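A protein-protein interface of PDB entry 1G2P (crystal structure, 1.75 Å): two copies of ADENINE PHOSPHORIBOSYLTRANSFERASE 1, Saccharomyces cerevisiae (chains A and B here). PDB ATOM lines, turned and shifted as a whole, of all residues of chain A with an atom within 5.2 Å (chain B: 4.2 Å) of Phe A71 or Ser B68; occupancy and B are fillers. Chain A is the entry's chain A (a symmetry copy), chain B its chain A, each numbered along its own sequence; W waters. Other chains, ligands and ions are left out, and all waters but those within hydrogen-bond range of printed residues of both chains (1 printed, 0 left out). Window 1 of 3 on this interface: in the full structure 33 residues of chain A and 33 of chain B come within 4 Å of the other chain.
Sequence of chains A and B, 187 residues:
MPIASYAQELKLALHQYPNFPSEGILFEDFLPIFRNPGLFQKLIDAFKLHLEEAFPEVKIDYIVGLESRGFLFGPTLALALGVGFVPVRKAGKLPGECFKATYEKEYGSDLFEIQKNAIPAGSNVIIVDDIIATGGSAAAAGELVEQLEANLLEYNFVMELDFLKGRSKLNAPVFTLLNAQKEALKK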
ATOM      1  N   GLY A  65      -5.166  -4.504 -10.379  1.00  0.00           N
ATOM      2  CA  GLY A  65      -4.096  -5.259 -11.009  1.00  0.00           C
ATOM      3  C   GLY A  65      -3.043  -4.397 -11.680  1.00  0.00           C
ATOM      4  O   GLY A  65      -3.358  -3.389 -12.309  1.00  0.00           O
ATOM      5  N   LEU A  66      -1.788  -4.814 -11.553  1.00  0.00           N
ATOM      6  CA  LEU A  66      -0.670  -4.083 -12.145  1.00  0.00           C
ATOM      7  C   LEU A  66      -0.402  -4.500 -13.586  1.00  0.00           C
ATOM      8  O   LEU A  66      -0.412  -5.683 -13.934  1.00  0.00           O
ATOM      9  CB  LEU A  66       0.599  -4.295 -11.315  1.00  0.00           C
ATOM     10  CG  LEU A  66       0.497  -4.112  -9.795  1.00  0.00           C
ATOM     11  CD1 LEU A  66       1.912  -4.018  -9.209  1.00  0.00           C
ATOM     12  CD2 LEU A  66      -0.298  -2.850  -9.461  1.00  0.00           C
ATOM     13  N   GLU A  67      -0.144  -3.511 -14.430  1.00  0.00           N
ATOM     14  CA  GLU A  67       0.141  -3.751 -15.845  1.00  0.00           C
ATOM     15  C   GLU A  67       1.518  -4.410 -16.009  1.00  0.00           C
ATOM     16  O   GLU A  67       2.483  -3.985 -15.367  1.00  0.00           O
ATOM     17  CB  GLU A  67       0.115  -2.420 -16.596  1.00  0.00           C
ATOM     18  CG  GLU A  67       0.467  -2.527 -18.064  1.00  0.00           C
ATOM     19  CD  GLU A  67       0.170  -1.258 -18.824  1.00  0.00           C
ATOM     20  OE1 GLU A  67      -0.154  -0.229 -18.195  1.00  0.00           O
ATOM     21  OE2 GLU A  67       0.256  -1.287 -20.065  1.00  0.00           O
ATOM     22  N   SER A  68       1.624  -5.436 -16.859  1.00  0.00           N
ATOM     23  CA  SER A  68       0.494  -5.954 -17.632  1.00  0.00           C
ATOM     24  C   SER A  68       0.157  -7.367 -17.187  1.00  0.00           C
ATOM     25  O   SER A  68      -0.946  -7.845 -17.428  1.00  0.00           O
ATOM     26  CB  SER A  68       0.790  -5.982 -19.137  1.00  0.00           C
ATOM     27  OG  SER A  68       1.987  -5.313 -19.443  1.00  0.00           O
ATOM     28  N   ARG A  69       1.097  -8.019 -16.503  1.00  0.00           N
ATOM     29  CA  ARG A  69       0.870  -9.396 -16.061  1.00  0.00           C
ATOM     30  C   ARG A  69      -0.218  -9.522 -15.018  1.00  0.00           C
ATOM     31  O   ARG A  69      -0.863 -10.570 -14.916  1.00  0.00           O
ATOM     32  CB  ARG A  69       2.168 -10.022 -15.545  1.00  0.00           C
ATOM     33  CG  ARG A  69       3.193 -10.238 -16.645  1.00  0.00           C
ATOM     34  CD  ARG A  69       4.355 -11.035 -16.106  1.00  0.00           C
ATOM     35  NE  ARG A  69       5.536 -10.960 -16.953  1.00  0.00           N
ATOM     36  CZ  ARG A  69       6.682 -10.401 -16.574  1.00  0.00           C
ATOM     37  NH1 ARG A  69       6.796  -9.865 -15.363  1.00  0.00           N
ATOM     38  NH2 ARG A  69       7.716 -10.390 -17.407  1.00  0.00           N
ATOM     39  N   GLY A  70      -0.417  -8.467 -14.237  1.00  0.00           N
ATOM     40  CA  GLY A  70      -1.476  -8.485 -13.245  1.00  0.00           C
ATOM     41  C   GLY A  70      -2.817  -8.460 -13.970  1.00  0.00           C
ATOM     42  O   GLY A  70      -3.837  -8.856 -13.417  1.00  0.00           O
ATOM     43  N   PHE A  71      -2.820  -7.989 -15.215  1.00  0.00           N
ATOM     44  CA  PHE A  71      -4.056  -7.947 -16.007  1.00  0.00           C
ATOM     45  C   PHE A  71      -4.491  -9.345 -16.461  1.00  0.00           C
ATOM     46  O   PHE A  71      -5.654  -9.558 -16.798  1.00  0.00           O
ATOM     47  CB  PHE A  71      -3.877  -7.141 -17.301  1.00  0.00           C
ATOM     48  CG  PHE A  71      -3.667  -5.658 -17.112  1.00  0.00           C
ATOM     49  CD1 PHE A  71      -3.603  -5.079 -15.847  1.00  0.00           C
ATOM     50  CD2 PHE A  71      -3.566  -4.836 -18.235  1.00  0.00           C
ATOM     51  CE1 PHE A  71      -3.445  -3.696 -15.697  1.00  0.00           C
ATOM     52  CE2 PHE A  71      -3.408  -3.451 -18.102  1.00  0.00           C
ATOM     53  CZ  PHE A  71      -3.348  -2.881 -16.827  1.00  0.00           C
ATOM     54  N   LEU A  72      -3.552 -10.285 -16.500  1.00  0.00           N
ATOM     55  CA  LEU A  72      -3.857 -11.626 -16.987  1.00  0.00           C
ATOM     56  C   LEU A  72      -4.766 -12.443 -16.073  1.00  0.00           C
ATOM     57  O   LEU A  72      -5.554 -13.257 -16.562  1.00  0.00           O
ATOM     58  CB  LEU A  72      -2.553 -12.385 -17.285  1.00  0.00           C
ATOM     59  CG  LEU A  72      -1.726 -11.789 -18.438  1.00  0.00           C
ATOM     60  CD1 LEU A  72      -0.318 -12.369 -18.399  1.00  0.00           C
ATOM     61  CD2 LEU A  72      -2.408 -12.062 -19.793  1.00  0.00           C
ATOM     62  N   PHE A  73      -4.685 -12.223 -14.765  1.00  0.00           N
ATOM     63  CA  PHE A  73      -5.539 -12.968 -13.843  1.00  0.00           C
ATOM     64  C   PHE A  73      -6.383 -12.083 -12.933  1.00  0.00           C
ATOM     65  O   PHE A  73      -7.383 -12.538 -12.394  1.00  0.00           O
ATOM     66  CB  PHE A  73      -4.713 -13.957 -12.987  1.00  0.00           C
ATOM     67  CG  PHE A  73      -3.822 -13.307 -11.943  1.00  0.00           C
ATOM     68  CD1 PHE A  73      -2.564 -12.825 -12.278  1.00  0.00           C
ATOM     69  CD2 PHE A  73      -4.243 -13.208 -10.616  1.00  0.00           C
ATOM     70  CE1 PHE A  73      -1.728 -12.257 -11.294  1.00  0.00           C
ATOM     71  CE2 PHE A  73      -3.427 -12.645  -9.625  1.00  0.00           C
ATOM     72  CZ  PHE A  73      -2.164 -12.169  -9.969  1.00  0.00           C
ATOM     73  N   GLY A  74      -5.994 -10.820 -12.785  1.00  0.00           N
ATOM     74  CA  GLY A  74      -6.727  -9.903 -11.912  1.00  0.00           C
ATOM     75  C   GLY A  74      -8.195  -9.732 -12.243  1.00  0.00           C
ATOM     76  O   GLY A  74      -9.052  -9.879 -11.360  1.00  0.00           O
ATOM     77  N   PRO A  75      -8.532  -9.384 -13.501  1.00  0.00           N
ATOM     78  CA  PRO A  75      -9.943  -9.217 -13.863  1.00  0.00           C
ATOM     79  C   PRO A  75     -10.733 -10.499 -13.633  1.00  0.00           C
ATOM     80  O   PRO A  75     -11.864 -10.466 -13.138  1.00  0.00           O
ATOM     81  CB  PRO A  75      -9.887  -8.857 -15.345  1.00  0.00           C
ATOM     82  CG  PRO A  75      -8.571  -8.109 -15.450  1.00  0.00           C
ATOM     83  CD  PRO A  75      -7.644  -8.955 -14.592  1.00  0.00           C
ATOM     84  N   PHE A  85     -12.819  -4.514 -10.886  1.00  0.00           N
ATOM     85  CA  PHE A  85     -11.408  -4.533 -11.230  1.00  0.00           C
ATOM     86  C   PHE A  85     -11.019  -3.157 -11.753  1.00  0.00           C
ATOM     87  O   PHE A  85     -11.754  -2.556 -12.543  1.00  0.00           O
ATOM     88  CB  PHE A  85     -11.116  -5.557 -12.332  1.00  0.00           C
ATOM     89  CG  PHE A  85      -9.680  -5.539 -12.776  1.00  0.00           C
ATOM     90  CD1 PHE A  85      -8.718  -6.264 -12.079  1.00  0.00           C
ATOM     91  CD2 PHE A  85      -9.277  -4.710 -13.820  1.00  0.00           C
ATOM     92  CE1 PHE A  85      -7.373  -6.163 -12.408  1.00  0.00           C
ATOM     93  CE2 PHE A  85      -7.920  -4.593 -14.169  1.00  0.00           C
ATOM     94  CZ  PHE A  85      -6.966  -5.319 -13.461  1.00  0.00           C
ATOM     95  N   PRO A  87      -7.293  -1.082 -13.079  1.00  0.00           N
ATOM     96  CA  PRO A  87      -5.872  -1.282 -13.355  1.00  0.00           C
ATOM     97  C   PRO A  87      -4.962  -0.135 -12.929  1.00  0.00           C
ATOM     98  O   PRO A  87      -5.395   1.013 -12.823  1.00  0.00           O
ATOM     99  CB  PRO A  87      -5.853  -1.433 -14.865  1.00  0.00           C
ATOM    100  CG  PRO A  87      -6.865  -0.338 -15.275  1.00  0.00           C
ATOM    101  CD  PRO A  87      -8.002  -0.599 -14.281  1.00  0.00           C
ATOM    102  N   VAL A  88      -3.715  -0.477 -12.640  1.00  0.00           N
ATOM    103  CA  VAL A  88      -2.696   0.535 -12.374  1.00  0.00           C
ATOM    104  C   VAL A  88      -1.904   0.392 -13.681  1.00  0.00           C
ATOM    105  O   VAL A  88      -1.487  -0.709 -14.057  1.00  0.00           O
ATOM    106  CB  VAL A  88      -1.800   0.198 -11.173  1.00  0.00           C
ATOM    107  CG1 VAL A  88      -0.518   1.075 -11.200  1.00  0.00           C
ATOM    108  CG2 VAL A  88      -2.561   0.467  -9.883  1.00  0.00           C
ATOM    109  N   ARG A  89      -1.718   1.489 -14.395  1.00  0.00           N
ATOM    110  CA  ARG A  89      -1.012   1.418 -15.656  1.00  0.00           C
ATOM    111  C   ARG A  89       0.258   2.236 -15.670  1.00  0.00           C
ATOM    112  O   ARG A  89       0.458   3.117 -14.822  1.00  0.00           O
ATOM    113  CB  ARG A  89      -1.925   1.898 -16.797  1.00  0.00           C
ATOM    114  CG  ARG A  89      -3.168   1.043 -17.026  1.00  0.00           C
ATOM    115  CD  ARG A  89      -3.606   1.072 -18.493  1.00  0.00           C
ATOM    116  NE  ARG A  89      -2.588   0.487 -19.366  1.00  0.00           N
ATOM    117  CZ  ARG A  89      -2.702   0.368 -20.687  1.00  0.00           C
ATOM    118  NH1 ARG A  89      -3.795   0.783 -21.305  1.00  0.00           N
ATOM    119  NH2 ARG A  89      -1.705  -0.147 -21.399  1.00  0.00           N
ATOM    120  N   LEU B  66      -4.209  -9.278 -27.312  1.00  0.00           N
ATOM    121  CA  LEU B  66      -3.156  -8.290 -27.540  1.00  0.00           C
ATOM    122  C   LEU B  66      -2.878  -7.441 -26.305  1.00  0.00           C
ATOM    123  O   LEU B  66      -3.790  -6.988 -25.609  1.00  0.00           O
ATOM    124  CB  LEU B  66      -3.535  -7.374 -28.706  1.00  0.00           C
ATOM    125  CG  LEU B  66      -4.033  -8.032 -30.000  1.00  0.00           C
ATOM    126  CD1 LEU B  66      -4.015  -6.991 -31.127  1.00  0.00           C
ATOM    127  CD2 LEU B  66      -3.150  -9.225 -30.367  1.00  0.00           C
ATOM    128  N   GLU B  67      -1.600  -7.213 -26.041  1.00  0.00           N
ATOM    129  CA  GLU B  67      -1.174  -6.410 -24.896  1.00  0.00           C
ATOM    130  C   GLU B  67      -1.514  -4.931 -25.123  1.00  0.00           C
ATOM    131  O   GLU B  67      -1.282  -4.407 -26.217  1.00  0.00           O
ATOM    132  CB  GLU B  67       0.335  -6.567 -24.705  1.00  0.00           C
ATOM    133  CG  GLU B  67       0.912  -5.725 -23.588  1.00  0.00           C
ATOM    134  CD  GLU B  67       2.333  -6.104 -23.253  1.00  0.00           C
ATOM    135  OE1 GLU B  67       2.943  -6.906 -23.990  1.00  0.00           O
ATOM    136  OE2 GLU B  67       2.848  -5.598 -22.239  1.00  0.00           O
ATOM    137  N   SER B  68      -2.055  -4.249 -24.109  1.00  0.00           N
ATOM    138  CA  SER B  68      -2.336  -4.848 -22.803  1.00  0.00           C
ATOM    139  C   SER B  68      -3.834  -4.889 -22.554  1.00  0.00           C
ATOM    140  O   SER B  68      -4.303  -5.654 -21.720  1.00  0.00           O
ATOM    141  CB  SER B  68      -1.680  -4.066 -21.658  1.00  0.00           C
ATOM    142  OG  SER B  68      -0.795  -3.086 -22.138  1.00  0.00           O
ATOM    143  N   ARG B  69      -4.587  -4.088 -23.309  1.00  0.00           N
ATOM    144  CA  ARG B  69      -6.037  -4.039 -23.117  1.00  0.00           C
ATOM    145  C   ARG B  69      -6.737  -5.329 -23.485  1.00  0.00           C
ATOM    146  O   ARG B  69      -7.803  -5.635 -22.941  1.00  0.00           O
ATOM    147  CB  ARG B  69      -6.649  -2.871 -23.893  1.00  0.00           C
ATOM    148  CG  ARG B  69      -6.239  -1.517 -23.335  1.00  0.00           C
ATOM    149  CD  ARG B  69      -7.031  -0.428 -24.013  1.00  0.00           C
ATOM    150  NE  ARG B  69      -6.449   0.894 -23.833  1.00  0.00           N
ATOM    151  CZ  ARG B  69      -5.962   1.628 -24.828  1.00  0.00           C
ATOM    152  NH1 ARG B  69      -5.984   1.164 -26.075  1.00  0.00           N
ATOM    153  NH2 ARG B  69      -5.461   2.832 -24.575  1.00  0.00           N
ATOM    154  N   GLY B  70      -6.153  -6.078 -24.411  1.00  0.00           N
ATOM    155  CA  GLY B  70      -6.730  -7.356 -24.785  1.00  0.00           C
ATOM    156  C   GLY B  70      -6.573  -8.319 -23.613  1.00  0.00           C
ATOM    157  O   GLY B  70      -7.295  -9.303 -23.507  1.00  0.00           O
ATOM    158  N   PHE B  71      -5.620  -8.038 -22.727  1.00  0.00           N
ATOM    159  CA  PHE B  71      -5.405  -8.888 -21.549  1.00  0.00           C
ATOM    160  C   PHE B  71      -6.519  -8.716 -20.510  1.00  0.00           C
ATOM    161  O   PHE B  71      -6.717  -9.581 -19.659  1.00  0.00           O
ATOM    162  CB  PHE B  71      -4.108  -8.525 -20.813  1.00  0.00           C
ATOM    163  CG  PHE B  71      -2.834  -8.833 -21.562  1.00  0.00           C
ATOM    164  CD1 PHE B  71      -2.848  -9.372 -22.846  1.00  0.00           C
ATOM    165  CD2 PHE B  71      -1.606  -8.602 -20.941  1.00  0.00           C
ATOM    166  CE1 PHE B  71      -1.654  -9.685 -23.506  1.00  0.00           C
ATOM    167  CE2 PHE B  71      -0.403  -8.910 -21.589  1.00  0.00           C
ATOM    168  CZ  PHE B  71      -0.430  -9.454 -22.877  1.00  0.00           C
ATOM    169  N   LEU B  72      -7.221  -7.589 -20.560  1.00  0.00           N
ATOM    170  CA  LEU B  72      -8.253  -7.307 -19.568  1.00  0.00           C
ATOM    171  C   LEU B  72      -9.492  -8.191 -19.670  1.00  0.00           C
ATOM    172  O   LEU B  72     -10.115  -8.493 -18.648  1.00  0.00           O
ATOM    173  CB  LEU B  72      -8.635  -5.817 -19.618  1.00  0.00           C
ATOM    174  CG  LEU B  72      -7.502  -4.862 -19.206  1.00  0.00           C
ATOM    175  CD1 LEU B  72      -7.854  -3.446 -19.644  1.00  0.00           C
ATOM    176  CD2 LEU B  72      -7.256  -4.934 -17.686  1.00  0.00           C
HETATM  177  O   HOH W   1      -6.499   2.155 -20.708  1.00  0.00           O
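OE2 of Glu B67 is in hydrogen-bond range of OG of Ser A68 (2.9 Å). The side-chain carboxylate of Glu A67 lies within hydrogen-bond range of the side-chain hydroxyl of Ser B68, 2.9 Å away. NH2 of Arg A89 lies within hydrogen-bond range of OG of Ser B68 (3.2 Å). The backbone carbonyl oxygen of Phe A71 sits close to the backbone carbonyl oxygen of Phe B71 (3.1 Å).
The backbone carbonyl oxygen of Val A88 sits at hydrogen-bond distance from the backbone NH of Glu A67, at 3.1 Å. NH2 of Arg A89 lies within salt-bridge range of OE2 of Glu A67 (2.6 Å).
Ser A68 touches Phe B71. Phe A71 touches Ser B68 (CD2 to O, 3.7 Å). Phe A71 touches Leu B72 (CG to CD2, 3.7 Å). Phe B71 touches Leu A72 (CG to CD2, 3.7 Å). CB of Pro A75 touches O of Leu B72 (3.3 Å). CD2 of Leu B72 touches CE2 of Phe A85, 3.6 Å away. Arg A89 touches Arg B69.
Leu A66 touches none of the printed residues of chain B. Printed residues of chain B within 4 Å of Ser A68: Glu B67 (2.9 Å) and Phe B71 (3.7 Å). Of chain B, only Ser B68, Phe B71 and Leu B72 come within 4 Å of Phe A71. Of the printed residues of chain B, Pro A75 touches Leu B72 (3.3 Å). Of the printed residues of chain B, Phe A85 touches Leu B72 (3.6 Å). Gly B70 touches none of the printed residues of chain A. Of the printed residues of chain A, Phe B71 touches Ser A68 (3.7 Å), Phe A71 (3.1 Å) and Leu A72 (3.7 Å). The nearest printed residue of chain A that does not touch Ser B68 is Ser A68 (4.02 Å). The nearest printed residue of chain B that does not touch Leu A72 is Leu B72 (6.1 Å).
Of the 15 printed residues of chain A, 7 touch a printed residue of chain B. Hydrophobic or aromatic side chains of chain A that line the printed part of chain B: Phe A71, Leu A72, Pro A75 and Phe A85. Hydrophobic or aromatic side chains of chain B that line the printed part of chain A: Phe B71 and Leu B72. Along chain B the printed residues that touch a printed residue of chain A span positions 67 to 72. Among the printed residues, 11 pairs touch across the chains. Among the printed residues, no Asp or Glu carboxylate lies within 4 Å of a Lys or Arg side-chain nitrogen of the other chain.
Glu A67 touches Ser B68, and with the chains exchanged Ser A68 touches Glu B67. Ser A68 touches Phe B71, and with the chains exchanged Phe A71 touches Ser B68. Phe B71 touches its own counterpart, Phe A71. Phe A71 touches Leu B72, and with the chains exchanged Leu A72 touches Phe B71.
Water W1 bridges NH1 of Arg A89 (3.1 Å) and NE of Arg B69 (3.4 Å).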
